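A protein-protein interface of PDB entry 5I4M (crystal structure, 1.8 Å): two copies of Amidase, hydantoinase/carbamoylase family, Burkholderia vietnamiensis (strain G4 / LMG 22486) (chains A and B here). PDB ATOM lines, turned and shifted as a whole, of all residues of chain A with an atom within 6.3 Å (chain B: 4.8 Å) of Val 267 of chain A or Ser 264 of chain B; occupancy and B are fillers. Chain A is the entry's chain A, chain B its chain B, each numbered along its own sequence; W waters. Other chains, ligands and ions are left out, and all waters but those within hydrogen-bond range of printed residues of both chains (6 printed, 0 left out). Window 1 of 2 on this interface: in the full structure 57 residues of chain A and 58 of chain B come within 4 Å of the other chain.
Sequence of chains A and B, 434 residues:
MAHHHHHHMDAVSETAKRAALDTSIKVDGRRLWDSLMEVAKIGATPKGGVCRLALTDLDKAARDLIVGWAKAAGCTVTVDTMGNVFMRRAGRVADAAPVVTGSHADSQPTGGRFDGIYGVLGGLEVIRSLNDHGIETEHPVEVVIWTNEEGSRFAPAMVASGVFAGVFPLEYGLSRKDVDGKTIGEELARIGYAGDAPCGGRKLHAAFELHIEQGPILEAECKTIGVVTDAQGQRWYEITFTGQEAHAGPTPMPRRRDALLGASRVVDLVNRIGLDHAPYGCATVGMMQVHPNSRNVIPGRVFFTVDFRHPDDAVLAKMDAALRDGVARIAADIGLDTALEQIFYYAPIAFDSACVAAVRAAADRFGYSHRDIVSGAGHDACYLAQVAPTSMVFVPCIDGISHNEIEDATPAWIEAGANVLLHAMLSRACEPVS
Ser 264 of chain B touches its own counterpart, Ser 264 of chain A.
Ser 264 of chain A touches Val 267 of chain B, and with the chains exchanged Val 267 of chain A touches Ser 264 of chain B.
Arg 265 of chain A touches Asp 268 of chain B, and with the chains exchanged Asp 268 of chain A touches Arg 265 of chain B.
Positions printed for both chains: 262, 263, 264, 265, 266, 267 and 268.
Of the 11 pairs that touch across the chains among the printed residues, 5 have their exchanged pair printed and touching as well.
The side-chain carboxylate (OD1) of Asp 268 of chain A lies within salt-bridge range of the guanidinium group (NE) of Arg 265 of chain B, 3.0 Å away.
OD1 of Asp 268 of chain B is in salt-bridge range of NE of Arg 265 of chain A, 2.8 Å away.
CB of Ser 264 of chain A touches O of Ser 264 of chain B, at 3.5 Å.
Ser 264 of chain A touches Val 267 of chain B (OG to CB, 3.4 Å).
Val 267 of chain A touches Leu 260 of chain B (CG1 to O, 3.9 Å).
Leu 261 of chain B touches Val 267 of chain A.
Ser 264 of chain B touches Val 267 of chain A (OG to CB, 3.3 Å).
CD1 of Leu 261 of chain B touches OD1 of Asp 268 of chain A, at 3.6 Å.
Asn 271 of chain A touches Leu 261 of chain B.
Asn 271 of chain A touches Arg 265 of chain B (ND2 to NH2, 3.7 Å).
Leu 260 of chain B touches Val 285 of chain A (CD2 to O, 3.5 Å).
The side-chain hydroxyl of Ser 264 of chain B lies within hydrogen-bond range of the backbone carbonyl oxygen of Leu 260 of chain B.
Water W6 lies within hydrogen-bond range of the side-chain amide nitrogen of Asn 271 of chain A (2.7 Å) and the guanidinium group of Arg 265 of chain B (3.0 Å).
Water W2 bridges OD2 of Asp 268 of chain B (2.7 Å) and NE of Arg 265 of chain A (3.4 Å).
Water W1 bridges O of Ser 264 of chain B (2.8 Å) and O of Ser 264 of chain A (2.9 Å).
Water W5 lies within hydrogen-bond range of ND2 of Asn 271 of chain A (2.8 Å), OD1 of Asp 268 of chain A (2.9 Å) and NH2 of Arg 265 of chain B (3.0 Å).
Water W4 bridges the side-chain carboxylate of Asp 268 of chain A (2.9 Å) and the side-chain carboxylate of Asp 268 of chain B (3.2 Å).
Water W3 bridges O of Asp 268 of chain B (3.0 Å) and NH2 of Arg 265 of chain A (3.1 Å).
Printed residues of chain B within 4 Å of Val 267 of chain A: Leu 260 (3.9 Å), Leu 261 (3.9 Å) and Ser 264 (3.3 Å).
Of the printed residues of chain A, Ser 264 of chain B touches Ser 264 and Val 267.
Printed residues of chain B within 4 Å of Asp 268 of chain A: Leu 261 (3.6 Å) and Arg 265 (3.0 Å).
Printed residues of chain A within 4 Å of Leu 261 of chain B: Val 267 (3.9 Å), Asp 268 (3.6 Å) and Asn 271 (3.7 Å).
Printed residues of chain B within 4 Å of Asn 271 of chain A: Leu 261 and Arg 265.
Printed residues of chain A within 4 Å of Val 267 of chain B: Ser 264 (3.4 Å).
Met 288 of chain A touches none of the printed residues of chain B.
Leu 269 of chain A touches none of the printed residues of chain B.
The nearest printed residue of chain B that does not touch Val 267 of chain A is Gly 262 of chain B (6.1 Å).
Printed residues of chain A that touch a printed residue of chain B: Ser 264, Arg 265, Val 267, Asp 268, Asn 271 and Val 285.
Among the printed residues, Asp or Glu carboxylates within 4 Å of a Lys or Arg side-chain nitrogen of the other chain: Arg 265 of chain A with Asp 268 of chain B (2.8 Å) and Asp 268 of chain A with Arg 265 of chain B (3.0 Å).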
ATOM      1  N   GLY A 262       8.823   3.214 -26.113  1.00  0.00           N
ATOM      2  CA  GLY A 262       7.465   3.537 -25.690  1.00  0.00           C
ATOM      3  C   GLY A 262       6.474   2.457 -26.075  1.00  0.00           C
ATOM      4  O   GLY A 262       5.699   1.980 -25.241  1.00  0.00           O
ATOM      5  N   ALA A 263       6.488   2.055 -27.349  1.00  0.00           N
ATOM      6  CA  ALA A 263       5.552   1.030 -27.802  1.00  0.00           C
ATOM      7  C   ALA A 263       5.723  -0.259 -27.011  1.00  0.00           C
ATOM      8  O   ALA A 263       4.736  -0.900 -26.629  1.00  0.00           O
ATOM      9  CB  ALA A 263       5.741   0.770 -29.298  1.00  0.00           C
ATOM     10  N   SER A 264       6.971  -0.658 -26.761  1.00  0.00           N
ATOM     11  CA  SER A 264       7.226  -1.874 -25.996  1.00  0.00           C
ATOM     12  C   SER A 264       6.670  -1.769 -24.583  1.00  0.00           C
ATOM     13  O   SER A 264       6.151  -2.749 -24.030  1.00  0.00           O
ATOM     14  CB  SER A 264       8.729  -2.156 -25.953  1.00  0.00           C
ATOM     15  OG  SER A 264       9.189  -2.486 -27.248  1.00  0.00           O
ATOM     16  N   ARG A 265       6.781  -0.594 -23.973  1.00  0.00           N
ATOM     17  CA  ARG A 265       6.203  -0.447 -22.644  1.00  0.00           C
ATOM     18  C   ARG A 265       4.686  -0.555 -22.687  1.00  0.00           C
ATOM     19  O   ARG A 265       4.074  -1.030 -21.723  1.00  0.00           O
ATOM     20  CB  ARG A 265       6.654   0.874 -22.026  1.00  0.00           C
ATOM     21  CG  ARG A 265       8.094   0.775 -21.564  1.00  0.00           C
ATOM     22  CD  ARG A 265       8.647   2.093 -21.032  1.00  0.00           C
ATOM     23  NE  ARG A 265      10.031   1.908 -20.609  1.00  0.00           N
ATOM     24  CZ  ARG A 265      10.877   2.900 -20.358  1.00  0.00           C
ATOM     25  NH1 ARG A 265      10.477   4.164 -20.488  1.00  0.00           N
ATOM     26  NH2 ARG A 265      12.122   2.628 -19.987  1.00  0.00           N
ATOM     27  N   VAL A 266       4.064  -0.144 -23.797  1.00  0.00           N
ATOM     28  CA  VAL A 266       2.613  -0.284 -23.899  1.00  0.00           C
ATOM     29  C   VAL A 266       2.230  -1.741 -24.131  1.00  0.00           C
ATOM     30  O   VAL A 266       1.189  -2.196 -23.646  1.00  0.00           O
ATOM     31  CB  VAL A 266       2.046   0.633 -24.998  1.00  0.00           C
ATOM     32  CG1 VAL A 266       0.532   0.446 -25.123  1.00  0.00           C
ATOM     33  CG2 VAL A 266       2.359   2.102 -24.676  1.00  0.00           C
ATOM     34  N   VAL A 267       3.053  -2.498 -24.859  1.00  0.00           N
ATOM     35  CA  VAL A 267       2.779  -3.929 -25.000  1.00  0.00           C
ATOM     36  C   VAL A 267       2.689  -4.581 -23.626  1.00  0.00           C
ATOM     37  O   VAL A 267       1.776  -5.373 -23.347  1.00  0.00           O
ATOM     38  CB  VAL A 267       3.852  -4.600 -25.878  1.00  0.00           C
ATOM     39  CG1 VAL A 267       3.735  -6.133 -25.807  1.00  0.00           C
ATOM     40  CG2 VAL A 267       3.729  -4.137 -27.333  1.00  0.00           C
ATOM     41  N   ASP A 268       3.621  -4.230 -22.737  1.00  0.00           N
ATOM     42  CA  ASP A 268       3.614  -4.765 -21.378  1.00  0.00           C
ATOM     43  C   ASP A 268       2.412  -4.251 -20.594  1.00  0.00           C
ATOM     44  O   ASP A 268       1.764  -5.015 -19.866  1.00  0.00           O
ATOM     45  CB  ASP A 268       4.924  -4.388 -20.681  1.00  0.00           C
ATOM     46  CG  ASP A 268       5.390  -5.429 -19.678  1.00  0.00           C
ATOM     47  OD1 ASP A 268       4.889  -6.571 -19.704  1.00  0.00           O
ATOM     48  OD2 ASP A 268       6.287  -5.101 -18.873  1.00  0.00           O
ATOM     49  N   LEU A 269       2.096  -2.964 -20.738  1.00  0.00           N
ATOM     50  CA  LEU A 269       0.927  -2.401 -20.068  1.00  0.00           C
ATOM     51  C   LEU A 269      -0.363  -3.074 -20.530  1.00  0.00           C
ATOM     52  O   LEU A 269      -1.242  -3.380 -19.715  1.00  0.00           O
ATOM     53  CB  LEU A 269       0.861  -0.894 -20.325  1.00  0.00           C
ATOM     54  CG  LEU A 269      -0.437  -0.192 -19.916  1.00  0.00           C
ATOM     55  CD1 LEU A 269      -0.584  -0.198 -18.416  1.00  0.00           C
ATOM     56  CD2 LEU A 269      -0.474   1.228 -20.471  1.00  0.00           C
ATOM     57  N   VAL A 270      -0.499  -3.297 -21.837  1.00  0.00           N
ATOM     58  CA  VAL A 270      -1.698  -3.944 -22.369  1.00  0.00           C
ATOM     59  C   VAL A 270      -1.881  -5.318 -21.745  1.00  0.00           C
ATOM     60  O   VAL A 270      -2.985  -5.690 -21.329  1.00  0.00           O
ATOM     61  CB  VAL A 270      -1.617  -4.023 -23.903  1.00  0.00           C
ATOM     62  CG1 VAL A 270      -2.598  -5.063 -24.467  1.00  0.00           C
ATOM     63  CG2 VAL A 270      -1.870  -2.654 -24.500  1.00  0.00           C
ATOM     64  N   ASN A 271      -0.795  -6.092 -21.665  1.00  0.00           N
ATOM     65  CA  ASN A 271      -0.867  -7.397 -21.016  1.00  0.00           C
ATOM     66  C   ASN A 271      -1.267  -7.247 -19.557  1.00  0.00           C
ATOM     67  O   ASN A 271      -2.144  -7.966 -19.060  1.00  0.00           O
ATOM     68  CB  ASN A 271       0.475  -8.114 -21.146  1.00  0.00           C
ATOM     69  CG  ASN A 271       0.463  -9.502 -20.525  1.00  0.00           C
ATOM     70  OD1 ASN A 271      -0.042 -10.464 -21.117  1.00  0.00           O
ATOM     71  ND2 ASN A 271       1.030  -9.616 -19.338  1.00  0.00           N
ATOM     72  N   ARG A 272      -0.658  -6.286 -18.859  1.00  0.00           N
ATOM     73  CA  ARG A 272      -1.006  -6.071 -17.460  1.00  0.00           C
ATOM     74  C   ARG A 272      -2.490  -5.757 -17.308  1.00  0.00           C
ATOM     75  O   ARG A 272      -3.161  -6.277 -16.405  1.00  0.00           O
ATOM     76  CB  ARG A 272      -0.150  -4.938 -16.894  1.00  0.00           C
ATOM     77  CG  ARG A 272      -0.284  -4.726 -15.414  1.00  0.00           C
ATOM     78  CD  ARG A 272       0.453  -5.812 -14.678  1.00  0.00           C
ATOM     79  NE  ARG A 272      -0.435  -6.857 -14.183  1.00  0.00           N
ATOM     80  CZ  ARG A 272      -0.044  -8.104 -13.939  1.00  0.00           C
ATOM     81  NH1 ARG A 272      -0.914  -8.993 -13.479  1.00  0.00           N
ATOM     82  NH2 ARG A 272       1.213  -8.466 -14.175  1.00  0.00           N
ATOM     83  N   VAL A 285      -1.513  -6.976 -28.068  1.00  0.00           N
ATOM     84  CA  VAL A 285      -0.939  -6.171 -29.146  1.00  0.00           C
ATOM     85  C   VAL A 285      -0.502  -7.154 -30.223  1.00  0.00           C
ATOM     86  O   VAL A 285       0.445  -7.923 -30.021  1.00  0.00           O
ATOM     87  CB  VAL A 285       0.239  -5.308 -28.667  1.00  0.00           C
ATOM     88  CG1 VAL A 285       0.904  -4.611 -29.852  1.00  0.00           C
ATOM     89  CG2 VAL A 285      -0.252  -4.272 -27.664  1.00  0.00           C
ATOM     90  N   MET A 288       2.430  -4.435 -35.186  1.00  0.00           N
ATOM     91  CA  MET A 288       3.385  -3.382 -34.873  1.00  0.00           C
ATOM     92  C   MET A 288       4.213  -3.112 -36.119  1.00  0.00           C
ATOM     93  O   MET A 288       4.647  -4.050 -36.787  1.00  0.00           O
ATOM     94  CB  MET A 288       4.306  -3.777 -33.707  1.00  0.00           C
ATOM     95  CG  MET A 288       5.270  -2.658 -33.317  1.00  0.00           C
ATOM     96  SD  MET A 288       6.220  -2.965 -31.812  1.00  0.00           S
ATOM     97  CE  MET A 288       4.937  -2.754 -30.575  1.00  0.00           C
ATOM     98  N   PHE A 304       1.121   0.681 -33.705  1.00  0.00           N
ATOM     99  CA  PHE A 304       0.735  -0.629 -33.188  1.00  0.00           C
ATOM    100  C   PHE A 304      -0.743  -0.619 -32.820  1.00  0.00           C
ATOM    101  O   PHE A 304      -1.381   0.437 -32.732  1.00  0.00           O
ATOM    102  CB  PHE A 304       1.607  -1.061 -32.002  1.00  0.00           C
ATOM    103  CG  PHE A 304       1.530  -0.139 -30.817  1.00  0.00           C
ATOM    104  CD1 PHE A 304       2.289   1.020 -30.772  1.00  0.00           C
ATOM    105  CD2 PHE A 304       0.710  -0.438 -29.754  1.00  0.00           C
ATOM    106  CE1 PHE A 304       2.220   1.870 -29.678  1.00  0.00           C
ATOM    107  CE2 PHE A 304       0.634   0.408 -28.662  1.00  0.00           C
ATOM    108  CZ  PHE A 304       1.389   1.563 -28.631  1.00  0.00           C
ATOM    109  N   LEU B 260       5.672 -11.234 -28.913  1.00  0.00           N
ATOM    110  CA  LEU B 260       5.875  -9.790 -28.862  1.00  0.00           C
ATOM    111  C   LEU B 260       5.924  -9.295 -27.427  1.00  0.00           C
ATOM    112  O   LEU B 260       6.673  -8.362 -27.121  1.00  0.00           O
ATOM    113  CB  LEU B 260       4.776  -9.072 -29.653  1.00  0.00           C
ATOM    114  CG  LEU B 260       4.865  -7.543 -29.701  1.00  0.00           C
ATOM    115  CD1 LEU B 260       6.244  -7.116 -30.212  1.00  0.00           C
ATOM    116  CD2 LEU B 260       3.776  -6.973 -30.583  1.00  0.00           C
ATOM    117  N   LEU B 261       5.154  -9.908 -26.529  1.00  0.00           N
ATOM    118  CA  LEU B 261       5.335  -9.610 -25.114  1.00  0.00           C
ATOM    119  C   LEU B 261       6.777  -9.864 -24.698  1.00  0.00           C
ATOM    120  O   LEU B 261       7.396  -9.032 -24.024  1.00  0.00           O
ATOM    121  CB  LEU B 261       4.373 -10.444 -24.266  1.00  0.00           C
ATOM    122  CG  LEU B 261       4.399 -10.175 -22.758  1.00  0.00           C
ATOM    123  CD1 LEU B 261       3.998  -8.707 -22.463  1.00  0.00           C
ATOM    124  CD2 LEU B 261       3.515 -11.173 -22.005  1.00  0.00           C
ATOM    125  N   GLY B 262       7.343 -10.990 -25.124  1.00  0.00           N
ATOM    126  CA  GLY B 262       8.735 -11.264 -24.796  1.00  0.00           C
ATOM    127  C   GLY B 262       9.684 -10.243 -25.394  1.00  0.00           C
ATOM    128  O   GLY B 262      10.527  -9.675 -24.695  1.00  0.00           O
ATOM    129  N   ALA B 263       9.557  -9.995 -26.698  1.00  0.00           N
ATOM    130  CA  ALA B 263      10.430  -9.033 -27.367  1.00  0.00           C
ATOM    131  C   ALA B 263      10.320  -7.649 -26.744  1.00  0.00           C
ATOM    132  O   ALA B 263      11.327  -6.949 -26.593  1.00  0.00           O
ATOM    133  CB  ALA B 263      10.088  -8.960 -28.855  1.00  0.00           C
ATOM    134  N   SER B 264       9.103  -7.237 -26.376  1.00  0.00           N
ATOM    135  CA  SER B 264       8.916  -5.918 -25.776  1.00  0.00           C
ATOM    136  C   SER B 264       9.619  -5.818 -24.430  1.00  0.00           C
ATOM    137  O   SER B 264      10.180  -4.766 -24.087  1.00  0.00           O
ATOM    138  CB  SER B 264       7.422  -5.632 -25.633  1.00  0.00           C
ATOM    139  OG  SER B 264       6.816  -5.609 -26.917  1.00  0.00           O
ATOM    140  N   ARG B 265       9.594  -6.896 -23.652  1.00  0.00           N
ATOM    141  CA  ARG B 265      10.309  -6.899 -22.386  1.00  0.00           C
ATOM    142  C   ARG B 265      11.819  -6.821 -22.594  1.00  0.00           C
ATOM    143  O   ARG B 265      12.523  -6.227 -21.772  1.00  0.00           O
ATOM    144  CB  ARG B 265       9.916  -8.132 -21.574  1.00  0.00           C
ATOM    145  CG  ARG B 265       8.506  -8.010 -21.055  1.00  0.00           C
ATOM    146  CD  ARG B 265       8.029  -9.237 -20.313  1.00  0.00           C
ATOM    147  NE  ARG B 265       6.701  -8.967 -19.764  1.00  0.00           N
ATOM    148  CZ  ARG B 265       5.915  -9.879 -19.210  1.00  0.00           C
ATOM    149  NH1 ARG B 265       6.318 -11.137 -19.121  1.00  0.00           N
ATOM    150  NH2 ARG B 265       4.720  -9.524 -18.744  1.00  0.00           N
ATOM    151  N   VAL B 266      12.331  -7.391 -23.688  1.00  0.00           N
ATOM    152  CA  VAL B 266      13.759  -7.266 -23.973  1.00  0.00           C
ATOM    153  C   VAL B 266      14.108  -5.851 -24.429  1.00  0.00           C
ATOM    154  O   VAL B 266      15.192  -5.346 -24.112  1.00  0.00           O
ATOM    155  CB  VAL B 266      14.203  -8.325 -25.002  1.00  0.00           C
ATOM    156  CG1 VAL B 266      15.677  -8.146 -25.357  1.00  0.00           C
ATOM    157  CG2 VAL B 266      13.981  -9.710 -24.429  1.00  0.00           C
ATOM    158  N   VAL B 267      13.211  -5.170 -25.152  1.00  0.00           N
ATOM    159  CA  VAL B 267      13.489  -3.774 -25.506  1.00  0.00           C
ATOM    160  C   VAL B 267      13.697  -2.947 -24.244  1.00  0.00           C
ATOM    161  O   VAL B 267      14.631  -2.141 -24.152  1.00  0.00           O
ATOM    162  CB  VAL B 267      12.364  -3.186 -26.372  1.00  0.00           C
ATOM    163  CG1 VAL B 267      12.558  -1.655 -26.535  1.00  0.00           C
ATOM    164  CG2 VAL B 267      12.298  -3.868 -27.730  1.00  0.00           C
ATOM    165  N   ASP B 268      12.846  -3.158 -23.242  1.00  0.00           N
ATOM    166  CA  ASP B 268      12.997  -2.434 -21.984  1.00  0.00           C
ATOM    167  C   ASP B 268      14.259  -2.875 -21.251  1.00  0.00           C
ATOM    168  O   ASP B 268      14.984  -2.041 -20.689  1.00  0.00           O
ATOM    169  CB  ASP B 268      11.746  -2.644 -21.119  1.00  0.00           C
ATOM    170  CG  ASP B 268      11.480  -1.473 -20.167  1.00  0.00           C
ATOM    171  OD1 ASP B 268      11.716  -0.307 -20.548  1.00  0.00           O
ATOM    172  OD2 ASP B 268      11.032  -1.721 -19.033  1.00  0.00           O
HETATM  173  O   HOH W   1       8.451  -3.466 -22.355  1.00  0.00           O
HETATM  174  O   HOH W   2       9.841   0.201 -17.630  1.00  0.00           O
HETATM  175  O   HOH W   3      14.423   0.607 -19.302  1.00  0.00           O
HETATM  176  O   HOH W   4       8.518  -3.542 -19.921  1.00  0.00           O
HETATM  177  O   HOH W   5       2.572  -7.518 -18.254  1.00  0.00           O
HETATM  178  O   HOH W   6       2.516 -11.327 -17.956  1.00  0.00           O
